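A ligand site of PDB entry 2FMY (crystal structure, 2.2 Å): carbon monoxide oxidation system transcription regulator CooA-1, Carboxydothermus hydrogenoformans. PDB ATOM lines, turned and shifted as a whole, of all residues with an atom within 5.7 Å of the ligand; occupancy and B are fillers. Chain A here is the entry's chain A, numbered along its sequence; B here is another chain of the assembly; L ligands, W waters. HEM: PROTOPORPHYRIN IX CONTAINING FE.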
ATOM      1  N   ASN A  42     -18.565  14.305 -26.605  1.00  0.00           N
ATOM      2  CA  ASN A  42     -19.803  14.357 -25.803  1.00  0.00           C
ATOM      3  C   ASN A  42     -20.163  13.025 -25.137  1.00  0.00           C
ATOM      4  O   ASN A  42     -21.292  12.540 -25.311  1.00  0.00           O
ATOM      5  CB  ASN A  42     -21.001  14.824 -26.651  1.00  0.00           C
ATOM      6  CG  ASN A  42     -20.806  16.198 -27.247  1.00  0.00           C
ATOM      7  OD1 ASN A  42     -20.588  17.181 -26.538  1.00  0.00           O
ATOM      8  ND2 ASN A  42     -20.931  16.286 -28.571  1.00  0.00           N
ATOM      9  N   VAL A  48     -15.411  17.407 -15.820  1.00  0.00           N
ATOM     10  CA  VAL A  48     -14.331  18.349 -15.962  1.00  0.00           C
ATOM     11  C   VAL A  48     -13.079  17.680 -15.416  1.00  0.00           C
ATOM     12  O   VAL A  48     -13.131  16.998 -14.384  1.00  0.00           O
ATOM     13  CB  VAL A  48     -14.640  19.711 -15.281  1.00  0.00           C
ATOM     14  CG1 VAL A  48     -13.399  20.633 -15.287  1.00  0.00           C
ATOM     15  CG2 VAL A  48     -15.821  20.379 -15.977  1.00  0.00           C
ATOM     16  N   ILE A  77      -6.990  22.499 -17.689  1.00  0.00           N
ATOM     17  CA  ILE A  77      -8.369  22.054 -17.529  1.00  0.00           C
ATOM     18  C   ILE A  77      -9.012  21.798 -18.895  1.00  0.00           C
ATOM     19  O   ILE A  77      -8.792  22.560 -19.839  1.00  0.00           O
ATOM     20  CB  ILE A  77      -9.226  23.122 -16.780  1.00  0.00           C
ATOM     21  CG1 ILE A  77      -8.774  23.320 -15.327  1.00  0.00           C
ATOM     22  CG2 ILE A  77     -10.700  22.802 -16.818  1.00  0.00           C
ATOM     23  CD1 ILE A  77      -9.120  22.165 -14.367  1.00  0.00           C
ATOM     24  N   PHE A  78      -9.796  20.734 -18.999  1.00  0.00           N
ATOM     25  CA  PHE A  78     -10.707  20.569 -20.123  1.00  0.00           C
ATOM     26  C   PHE A  78     -11.942  19.797 -19.673  1.00  0.00           C
ATOM     27  O   PHE A  78     -12.115  19.583 -18.476  1.00  0.00           O
ATOM     28  CB  PHE A  78     -10.006  19.935 -21.352  1.00  0.00           C
ATOM     29  CG  PHE A  78     -10.635  20.325 -22.664  1.00  0.00           C
ATOM     30  CD1 PHE A  78     -10.732  21.665 -23.040  1.00  0.00           C
ATOM     31  CD2 PHE A  78     -11.159  19.356 -23.514  1.00  0.00           C
ATOM     32  CE1 PHE A  78     -11.344  22.026 -24.234  1.00  0.00           C
ATOM     33  CE2 PHE A  78     -11.771  19.717 -24.708  1.00  0.00           C
ATOM     34  CZ  PHE A  78     -11.857  21.046 -25.066  1.00  0.00           C
ATOM     35  N   CYS A  79     -12.805  19.409 -20.601  1.00  0.00           N
ATOM     36  CA  CYS A  79     -14.071  18.765 -20.261  1.00  0.00           C
ATOM     37  C   CYS A  79     -14.433  17.690 -21.285  1.00  0.00           C
ATOM     38  O   CYS A  79     -13.751  17.507 -22.294  1.00  0.00           O
ATOM     39  CB  CYS A  79     -15.193  19.792 -20.183  1.00  0.00           C
ATOM     40  SG  CYS A  79     -15.630  20.456 -21.805  1.00  0.00           S
ATOM     41  N   HIS A  81     -17.617  17.557 -22.706  1.00  0.00           N
ATOM     42  CA  HIS A  81     -18.878  17.929 -23.383  1.00  0.00           C
ATOM     43  C   HIS A  81     -18.666  18.753 -24.661  1.00  0.00           C
ATOM     44  O   HIS A  81     -19.486  19.600 -25.021  1.00  0.00           O
ATOM     45  CB  HIS A  81     -19.910  18.569 -22.422  1.00  0.00           C
ATOM     46  CG  HIS A  81     -19.426  19.815 -21.749  1.00  0.00           C
ATOM     47  ND1 HIS A  81     -18.976  19.827 -20.442  1.00  0.00           N
ATOM     48  CD2 HIS A  81     -19.306  21.086 -22.204  1.00  0.00           C
ATOM     49  CE1 HIS A  81     -18.618  21.055 -20.118  1.00  0.00           C
ATOM     50  NE2 HIS A  81     -18.804  21.839 -21.161  1.00  0.00           N
ATOM     51  N   THR A  82     -17.561  18.470 -25.349  1.00  0.00           N
ATOM     52  CA  THR A  82     -17.254  19.119 -26.621  1.00  0.00           C
ATOM     53  C   THR A  82     -17.303  18.090 -27.755  1.00  0.00           C
ATOM     54  O   THR A  82     -17.289  16.884 -27.505  1.00  0.00           O
ATOM     55  CB  THR A  82     -15.851  19.801 -26.622  1.00  0.00           C
ATOM     56  OG1 THR A  82     -14.839  18.811 -26.839  1.00  0.00           O
ATOM     57  CG2 THR A  82     -15.581  20.539 -25.296  1.00  0.00           C
ATOM     58  N   ARG A  83     -17.322  18.577 -28.984  1.00  0.00           N
ATOM     59  CA  ARG A  83     -17.338  17.713 -30.168  1.00  0.00           C
ATOM     60  C   ARG A  83     -15.956  17.163 -30.573  1.00  0.00           C
ATOM     61  O   ARG A  83     -15.803  16.636 -31.677  1.00  0.00           O
ATOM     62  CB  ARG A  83     -17.999  18.435 -31.339  1.00  0.00           C
ATOM     63  CG  ARG A  83     -19.532  18.412 -31.278  1.00  0.00           C
ATOM     64  CD  ARG A  83     -20.130  19.470 -32.180  1.00  0.00           C
ATOM     65  NE  ARG A  83     -19.865  20.823 -31.684  1.00  0.00           N
ATOM     66  CZ  ARG A  83     -20.100  21.945 -32.357  1.00  0.00           C
ATOM     67  NH1 ARG A  83     -20.602  21.909 -33.594  1.00  0.00           N
ATOM     68  NH2 ARG A  83     -19.828  23.119 -31.795  1.00  0.00           N
ATOM     69  N   ALA A  84     -14.967  17.262 -29.694  1.00  0.00           N
ATOM     70  CA  ALA A  84     -13.609  16.820 -30.000  1.00  0.00           C
ATOM     71  C   ALA A  84     -13.260  15.479 -29.340  1.00  0.00           C
ATOM     72  O   ALA A  84     -13.868  15.091 -28.345  1.00  0.00           O
ATOM     73  CB  ALA A  84     -12.617  17.881 -29.582  1.00  0.00           C
ATOM     74  N   ILE A  99     -19.213  17.613 -13.654  1.00  0.00           N
ATOM     75  CA  ILE A  99     -19.460  19.032 -13.930  1.00  0.00           C
ATOM     76  C   ILE A  99     -20.284  19.750 -12.829  1.00  0.00           C
ATOM     77  O   ILE A  99     -20.138  20.959 -12.621  1.00  0.00           O
ATOM     78  CB  ILE A  99     -20.136  19.213 -15.337  1.00  0.00           C
ATOM     79  CG1 ILE A  99     -20.097  20.674 -15.791  1.00  0.00           C
ATOM     80  CG2 ILE A  99     -21.579  18.631 -15.341  1.00  0.00           C
ATOM     81  CD1 ILE A  99     -20.796  20.927 -17.129  1.00  0.00           C
ATOM     82  N   PHE A 102     -17.950  20.816 -10.290  1.00  0.00           N
ATOM     83  CA  PHE A 102     -17.069  21.854 -10.822  1.00  0.00           C
ATOM     84  C   PHE A 102     -17.739  23.219 -10.878  1.00  0.00           C
ATOM     85  O   PHE A 102     -17.062  24.255 -10.784  1.00  0.00           O
ATOM     86  CB  PHE A 102     -16.518  21.474 -12.211  1.00  0.00           C
ATOM     87  CG  PHE A 102     -15.341  22.316 -12.625  1.00  0.00           C
ATOM     88  CD1 PHE A 102     -14.113  22.173 -11.998  1.00  0.00           C
ATOM     89  CD2 PHE A 102     -15.474  23.265 -13.642  1.00  0.00           C
ATOM     90  CE1 PHE A 102     -13.015  22.946 -12.373  1.00  0.00           C
ATOM     91  CE2 PHE A 102     -14.380  24.042 -14.034  1.00  0.00           C
ATOM     92  CZ  PHE A 102     -13.152  23.889 -13.397  1.00  0.00           C
ATOM     93  N   GLN A 103     -19.057  23.222 -11.024  1.00  0.00           N
ATOM     94  CA  GLN A 103     -19.853  24.442 -11.018  1.00  0.00           C
ATOM     95  C   GLN A 103     -19.575  25.298  -9.773  1.00  0.00           C
ATOM     96  O   GLN A 103     -19.372  26.507  -9.884  1.00  0.00           O
ATOM     97  CB  GLN A 103     -21.352  24.105 -11.130  1.00  0.00           C
ATOM     98  CG  GLN A 103     -22.276  25.312 -11.074  1.00  0.00           C
ATOM     99  CD  GLN A 103     -22.108  26.232 -12.275  1.00  0.00           C
ATOM    100  OE1 GLN A 103     -22.583  25.933 -13.383  1.00  0.00           O
ATOM    101  NE2 GLN A 103     -21.437  27.356 -12.061  1.00  0.00           N
ATOM    102  N   VAL A 106     -15.529  26.392  -9.906  1.00  0.00           N
ATOM    103  CA  VAL A 106     -15.174  27.474 -10.821  1.00  0.00           C
ATOM    104  C   VAL A 106     -15.632  28.860 -10.334  1.00  0.00           C
ATOM    105  O   VAL A 106     -14.984  29.875 -10.604  1.00  0.00           O
ATOM    106  CB  VAL A 106     -15.634  27.167 -12.289  1.00  0.00           C
ATOM    107  CG1 VAL A 106     -17.124  27.474 -12.506  1.00  0.00           C
ATOM    108  CG2 VAL A 106     -14.740  27.925 -13.296  1.00  0.00           C
ATOM    109  N   MET A 116      -8.794  28.206 -17.676  1.00  0.00           N
ATOM    110  CA  MET A 116      -9.762  27.958 -18.733  1.00  0.00           C
ATOM    111  C   MET A 116      -9.665  28.974 -19.869  1.00  0.00           C
ATOM    112  O   MET A 116      -9.722  28.600 -21.033  1.00  0.00           O
ATOM    113  CB  MET A 116     -11.169  27.917 -18.141  1.00  0.00           C
ATOM    114  CG  MET A 116     -11.465  26.610 -17.405  1.00  0.00           C
ATOM    115  SD  MET A 116     -12.980  26.717 -16.443  1.00  0.00           S
ATOM    116  CE  MET A 116     -14.219  26.729 -17.737  1.00  0.00           C
ATOM    117  N   VAL A 119      -6.509  28.061 -21.921  1.00  0.00           N
ATOM    118  CA  VAL A 119      -6.816  26.886 -22.727  1.00  0.00           C
ATOM    119  C   VAL A 119      -7.787  27.211 -23.864  1.00  0.00           C
ATOM    120  O   VAL A 119      -7.502  26.908 -25.015  1.00  0.00           O
ATOM    121  CB  VAL A 119      -7.385  25.715 -21.847  1.00  0.00           C
ATOM    122  CG1 VAL A 119      -7.826  24.531 -22.737  1.00  0.00           C
ATOM    123  CG2 VAL A 119      -6.342  25.261 -20.835  1.00  0.00           C
ATOM    124  N   LEU A 120      -8.923  27.851 -23.551  1.00  0.00           N
ATOM    125  CA  LEU A 120      -9.929  28.156 -24.572  1.00  0.00           C
ATOM    126  C   LEU A 120      -9.397  29.125 -25.635  1.00  0.00           C
ATOM    127  O   LEU A 120      -9.732  28.996 -26.808  1.00  0.00           O
ATOM    128  CB  LEU A 120     -11.228  28.692 -23.969  1.00  0.00           C
ATOM    129  CG  LEU A 120     -12.130  27.740 -23.159  1.00  0.00           C
ATOM    130  CD1 LEU A 120     -13.250  28.527 -22.479  1.00  0.00           C
ATOM    131  CD2 LEU A 120     -12.705  26.582 -24.030  1.00  0.00           C
ATOM    132  N   LEU A 123      -7.179  26.994 -28.015  1.00  0.00           N
ATOM    133  CA  LEU A 123      -8.053  26.200 -28.900  1.00  0.00           C
ATOM    134  C   LEU A 123      -8.692  27.051 -29.991  1.00  0.00           C
ATOM    135  O   LEU A 123      -8.808  26.617 -31.137  1.00  0.00           O
ATOM    136  CB  LEU A 123      -9.176  25.525 -28.118  1.00  0.00           C
ATOM    137  CG  LEU A 123      -8.810  24.493 -27.058  1.00  0.00           C
ATOM    138  CD1 LEU A 123      -9.787  24.653 -25.912  1.00  0.00           C
ATOM    139  CD2 LEU A 123      -8.882  23.087 -27.647  1.00  0.00           C
ATOM    140  N   GLN B   3     -26.694  29.977 -22.653  1.00  0.00           N
ATOM    141  CA  GLN B   3     -26.283  28.633 -22.209  1.00  0.00           C
ATOM    142  C   GLN B   3     -24.808  28.434 -21.870  1.00  0.00           C
ATOM    143  O   GLN B   3     -24.452  27.452 -21.222  1.00  0.00           O
ATOM    144  CB  GLN B   3     -26.734  27.575 -23.235  1.00  0.00           C
ATOM    145  CG  GLN B   3     -28.133  26.995 -22.970  1.00  0.00           C
ATOM    146  CD  GLN B   3     -29.251  28.032 -23.083  1.00  0.00           C
ATOM    147  OE1 GLN B   3     -29.181  28.971 -23.880  1.00  0.00           O
ATOM    148  NE2 GLN B   3     -30.309  27.843 -22.287  1.00  0.00           N
ATOM    149  N   MET B   4     -23.966  29.371 -22.271  1.00  0.00           N
ATOM    150  CA  MET B   4     -22.533  29.271 -22.024  1.00  0.00           C
ATOM    151  C   MET B   4     -22.139  29.856 -20.657  1.00  0.00           C
ATOM    152  O   MET B   4     -20.974  29.812 -20.270  1.00  0.00           O
ATOM    153  CB  MET B   4     -21.755  29.954 -23.155  1.00  0.00           C
ATOM    154  CG  MET B   4     -20.465  29.241 -23.563  1.00  0.00           C
ATOM    155  SD  MET B   4     -20.663  27.618 -24.352  1.00  0.00           S
ATOM    156  CE  MET B   4     -21.510  28.068 -25.860  1.00  0.00           C
ATOM    157  N   ARG B   5     -23.125  30.382 -19.920  1.00  0.00           N
ATOM    158  CA  ARG B   5     -22.872  31.084 -18.655  1.00  0.00           C
ATOM    159  C   ARG B   5     -22.537  30.155 -17.490  1.00  0.00           C
ATOM    160  O   ARG B   5     -23.159  29.107 -17.311  1.00  0.00           O
ATOM    161  CB  ARG B   5     -24.036  32.038 -18.307  1.00  0.00           C
ATOM    162  CG  ARG B   5     -25.321  31.365 -17.840  1.00  0.00           C
ATOM    163  CD  ARG B   5     -26.450  32.362 -17.626  1.00  0.00           C
ATOM    164  NE  ARG B   5     -27.523  31.803 -16.787  1.00  0.00           N
ATOM    165  CZ  ARG B   5     -28.541  32.498 -16.286  1.00  0.00           C
ATOM    166  NH1 ARG B   5     -28.662  33.806 -16.528  1.00  0.00           N
ATOM    167  NH2 ARG B   5     -29.451  31.889 -15.537  1.00  0.00           N
ATOM    168  N   LEU B   6     -21.530  30.553 -16.711  1.00  0.00           N
ATOM    169  CA  LEU B   6     -21.143  29.802 -15.515  1.00  0.00           C
ATOM    170  C   LEU B   6     -21.757  30.412 -14.261  1.00  0.00           C
ATOM    171  O   LEU B   6     -21.680  29.832 -13.180  1.00  0.00           O
ATOM    172  CB  LEU B   6     -19.619  29.745 -15.379  1.00  0.00           C
ATOM    173  CG  LEU B   6     -18.755  29.248 -16.540  1.00  0.00           C
ATOM    174  CD1 LEU B   6     -17.305  29.146 -16.092  1.00  0.00           C
ATOM    175  CD2 LEU B   6     -19.251  27.923 -17.089  1.00  0.00           C
ATOM    176  N   GLY B 121     -15.904  30.154 -24.926  1.00  0.00           N
ATOM    177  CA  GLY B 121     -16.639  28.899 -25.159  1.00  0.00           C
ATOM    178  C   GLY B 121     -17.639  29.009 -26.293  1.00  0.00           C
ATOM    179  O   GLY B 121     -17.740  28.136 -27.145  1.00  0.00           O
ATOM    180  N   ASP B 122     -18.387  30.107 -26.329  1.00  0.00           N
ATOM    181  CA  ASP B 122     -19.292  30.379 -27.431  1.00  0.00           C
ATOM    182  C   ASP B 122     -18.590  30.538 -28.789  1.00  0.00           C
ATOM    183  O   ASP B 122     -19.042  29.957 -29.779  1.00  0.00           O
ATOM    184  CB  ASP B 122     -20.127  31.633 -27.131  1.00  0.00           C
ATOM    185  CG  ASP B 122     -21.329  31.757 -28.057  1.00  0.00           C
ATOM    186  OD1 ASP B 122     -21.649  32.910 -28.450  1.00  0.00           O
ATOM    187  OD2 ASP B 122     -21.956  30.720 -28.376  1.00  0.00           O
ATOM    188  N   LEU B 124     -15.664  29.286 -29.582  1.00  0.00           N
ATOM    189  CA  LEU B 124     -15.143  27.960 -29.927  1.00  0.00           C
ATOM    190  C   LEU B 124     -16.270  27.051 -30.439  1.00  0.00           C
ATOM    191  O   LEU B 124     -16.091  26.315 -31.416  1.00  0.00           O
ATOM    192  CB  LEU B 124     -14.385  27.321 -28.758  1.00  0.00           C
ATOM    193  CG  LEU B 124     -13.554  26.060 -29.064  1.00  0.00           C
ATOM    194  CD1 LEU B 124     -12.544  26.316 -30.157  1.00  0.00           C
ATOM    195  CD2 LEU B 124     -12.848  25.549 -27.827  1.00  0.00           C
ATOM    196  N   LYS B 125     -17.433  27.119 -29.789  1.00  0.00           N
ATOM    197  CA  LYS B 125     -18.602  26.358 -30.198  1.00  0.00           C
ATOM    198  C   LYS B 125     -18.954  26.639 -31.667  1.00  0.00           C
ATOM    199  O   LYS B 125     -19.157  25.702 -32.441  1.00  0.00           O
ATOM    200  CB  LYS B 125     -19.802  26.704 -29.311  1.00  0.00           C
ATOM    201  CG  LYS B 125     -20.998  25.778 -29.480  1.00  0.00           C
ATOM    202  CD  LYS B 125     -22.324  26.526 -29.288  1.00  0.00           C
ATOM    203  CE  LYS B 125     -22.563  27.484 -30.453  1.00  0.00           C
ATOM    204  NZ  LYS B 125     -23.838  28.265 -30.384  1.00  0.00           N
ATOM    205  N   ASN B 126     -19.038  27.910 -32.035  1.00  0.00           N
ATOM    206  CA  ASN B 126     -19.364  28.304 -33.398  1.00  0.00           C
ATOM    207  C   ASN B 126     -18.265  27.985 -34.393  1.00  0.00           C
ATOM    208  O   ASN B 126     -18.551  27.661 -35.541  1.00  0.00           O
ATOM    209  CB  ASN B 126     -19.751  29.774 -33.434  1.00  0.00           C
ATOM    210  CG  ASN B 126     -20.981  30.067 -32.584  1.00  0.00           C
ATOM    211  OD1 ASN B 126     -22.006  29.419 -32.740  1.00  0.00           O
ATOM    212  ND2 ASN B 126     -20.879  31.017 -31.667  1.00  0.00           N
ATOM    213  N   LEU B 128     -16.078  25.339 -34.234  1.00  0.00           N
ATOM    214  CA  LEU B 128     -16.198  23.914 -34.506  1.00  0.00           C
ATOM    215  C   LEU B 128     -17.312  23.599 -35.498  1.00  0.00           C
ATOM    216  O   LEU B 128     -17.134  22.781 -36.387  1.00  0.00           O
ATOM    217  CB  LEU B 128     -16.392  23.114 -33.201  1.00  0.00           C
ATOM    218  CG  LEU B 128     -15.332  23.290 -32.109  1.00  0.00           C
ATOM    219  CD1 LEU B 128     -15.550  22.296 -30.958  1.00  0.00           C
ATOM    220  CD2 LEU B 128     -13.912  23.231 -32.665  1.00  0.00           C
ATOM    221  N   LYS B 193     -26.994  21.997 -31.879  1.00  0.00           N
ATOM    222  CA  LYS B 193     -26.132  22.887 -31.088  1.00  0.00           C
ATOM    223  C   LYS B 193     -26.354  24.351 -31.464  1.00  0.00           C
ATOM    224  O   LYS B 193     -26.121  25.232 -30.645  1.00  0.00           O
ATOM    225  CB  LYS B 193     -24.655  22.507 -31.230  1.00  0.00           C
ATOM    226  CG  LYS B 193     -24.229  21.175 -30.582  1.00  0.00           C
ATOM    227  CD  LYS B 193     -23.962  21.286 -29.066  1.00  0.00           C
ATOM    228  CE  LYS B 193     -22.595  21.901 -28.759  1.00  0.00           C
ATOM    229  NZ  LYS B 193     -22.396  22.347 -27.335  1.00  0.00           N
HETATM  230  CHA HEM L   1     -20.241  23.860 -24.080  1.00  0.00           C
HETATM  231  CHB HEM L   1     -21.600  24.418 -19.464  1.00  0.00           C
HETATM  232  CHC HEM L   1     -16.987  23.746 -18.055  1.00  0.00           C
HETATM  233  CHD HEM L   1     -15.541  24.176 -22.689  1.00  0.00           C
HETATM  234  C1A HEM L   1     -21.032  24.011 -22.956  1.00  0.00           C
HETATM  235  C2A HEM L   1     -22.490  24.020 -22.913  1.00  0.00           C
HETATM  236  C3A HEM L   1     -22.874  24.183 -21.631  1.00  0.00           C
HETATM  237  C4A HEM L   1     -21.669  24.257 -20.825  1.00  0.00           C
HETATM  238  CMA HEM L   1     -24.343  24.254 -21.114  1.00  0.00           C
HETATM  239  CAA HEM L   1     -23.417  23.913 -24.153  1.00  0.00           C
HETATM  240  CBA HEM L   1     -23.689  25.356 -24.582  1.00  0.00           C
HETATM  241  CGA HEM L   1     -24.783  25.470 -25.614  1.00  0.00           C
HETATM  242  O1A HEM L   1     -25.935  25.037 -25.358  1.00  0.00           O
HETATM  243  O2A HEM L   1     -24.493  26.027 -26.703  1.00  0.00           O
HETATM  244  C1B HEM L   1     -20.468  24.338 -18.681  1.00  0.00           C
HETATM  245  C2B HEM L   1     -20.417  24.534 -17.249  1.00  0.00           C
HETATM  246  C3B HEM L   1     -19.138  24.346 -16.853  1.00  0.00           C
HETATM  247  C4B HEM L   1     -18.344  24.017 -18.028  1.00  0.00           C
HETATM  248  CMB HEM L   1     -21.647  24.913 -16.387  1.00  0.00           C
HETATM  249  CAB HEM L   1     -18.557  24.470 -15.433  1.00  0.00           C
HETATM  250  CBB HEM L   1     -19.276  24.236 -14.339  1.00  0.00           C
HETATM  251  C1C HEM L   1     -16.174  23.764 -19.180  1.00  0.00           C
HETATM  252  C2C HEM L   1     -14.742  23.536 -19.235  1.00  0.00           C
HETATM  253  C3C HEM L   1     -14.341  23.677 -20.516  1.00  0.00           C
HETATM  254  C4C HEM L   1     -15.513  23.976 -21.319  1.00  0.00           C
HETATM  255  CMC HEM L   1     -13.838  23.205 -18.020  1.00  0.00           C
HETATM  256  CAC HEM L   1     -12.908  23.528 -21.089  1.00  0.00           C
HETATM  257  CBC HEM L   1     -11.951  24.380 -20.714  1.00  0.00           C
HETATM  258  C1D HEM L   1     -16.648  24.086 -23.514  1.00  0.00           C
HETATM  259  C2D HEM L   1     -16.639  24.058 -24.971  1.00  0.00           C
HETATM  260  C3D HEM L   1     -18.100  23.969 -25.389  1.00  0.00           C
HETATM  261  C4D HEM L   1     -18.865  23.943 -24.168  1.00  0.00           C
HETATM  262  CMD HEM L   1     -15.406  24.127 -25.893  1.00  0.00           C
HETATM  263  CAD HEM L   1     -18.637  23.890 -26.834  1.00  0.00           C
HETATM  264  CBD HEM L   1     -18.542  22.420 -27.189  1.00  0.00           C
HETATM  265  CGD HEM L   1     -18.857  22.151 -28.637  1.00  0.00           C
HETATM  266  O1D HEM L   1     -18.509  21.064 -29.127  1.00  0.00           O
HETATM  267  O2D HEM L   1     -19.462  23.019 -29.305  1.00  0.00           O
HETATM  268  NA  HEM L   1     -20.572  24.151 -21.666  1.00  0.00           N
HETATM  269  NB  HEM L   1     -19.190  24.015 -19.117  1.00  0.00           N
HETATM  270  NC  HEM L   1     -16.604  24.010 -20.463  1.00  0.00           N
HETATM  271  ND  HEM L   1     -17.972  24.019 -23.101  1.00  0.00           N
HETATM  272 FE   HEM L   1     -18.566  23.983 -21.148  1.00  0.00          FE
HETATM  273  O   HOH W   1     -20.943  19.423 -27.823  1.00  0.00           O
HETATM  274  O   HOH W   2     -22.317  20.943 -20.256  1.00  0.00           O
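Water W1 lies within hydrogen-bond range of OD1 of Asn 42 (2.6 Å), O of His 81 (3.2 Å), O1D of the ligand (3.2 Å) and NZ of Lys 193 of chain B (3.3 Å).
The backbone NH (N) of His 81 lies close to the side-chain sulfur (SG) of Cys 79 (3.6 Å).
OD1 of Asn 42 lies close to O of His 81, at 3.1 Å.
NH2 of Arg 83 lies within hydrogen-bond range of O of Lys 125 of chain B.
The side-chain amino group (NZ) of Lys 125 of chain B lies within salt-bridge range of the side-chain carboxylate (OD2) of Asp 122 of chain B (3.7 Å).
NZ of Lys 125 of chain B lies close to OD1 of Asn 126 of chain B, 3.2 Å away.
The backbone carbonyl oxygen of Leu 6 of chain B lies within hydrogen-bond range of the side-chain amide nitrogen of Gln 103 (2.7 Å).
The backbone carbonyl oxygen of Thr 82 is in hydrogen-bond range of the backbone NH of Asn 42, at 3.0 Å.
The side-chain hydroxyl (OG1) of Thr 82 sits close to the backbone NH (N) of Ala 84.
Residues that only touch the ligand: Lys 125 of chain B (3.2 Å), Gln 3 of chain B (3.2 Å), Gln 103 (3.3 Å), Ile 77 (3.4 Å), Thr 82 (3.4 Å), Phe 78 (3.5 Å), Leu 124 of chain B (3.5 Å), Cys 79 (3.6 Å), Met 116 (3.6 Å), Leu 6 of chain B (3.6 Å), Ile 99 (3.6 Å), Leu 128 of chain B (3.7 Å), Met 4 of chain B (3.7 Å), Phe 102 (3.8 Å), Val 48 (3.8 Å) and Leu 120 (3.95 Å).
Hydrophobic or aromatic side chains within 4 Å of the ligand: Val 48, Ile 77, Phe 78, His 81, Ile 99, Phe 102, Met 116, Leu 120, Met 4 of chain B, Leu 6 of chain B, Leu 124 of chain B and Leu 128 of chain B.
The nearest printed residue that does not touch the ligand is Val 106 (4.3 Å).
A ring nitrogen (NE2) of His 81 binds an iron atom (FE) of the ligand, at 2.2 Å.
The backbone NH (N) of Arg 83 is in hydrogen-bond range of an oxygen (O1D) of the ligand.
O2D of the ligand is in salt-bridge range of NH2 of Arg 83 (2.5 Å).
An oxygen (O2D) of the ligand is in salt-bridge range of the side-chain amino group (NZ) of Lys 193 of chain B, 3.6 Å away.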
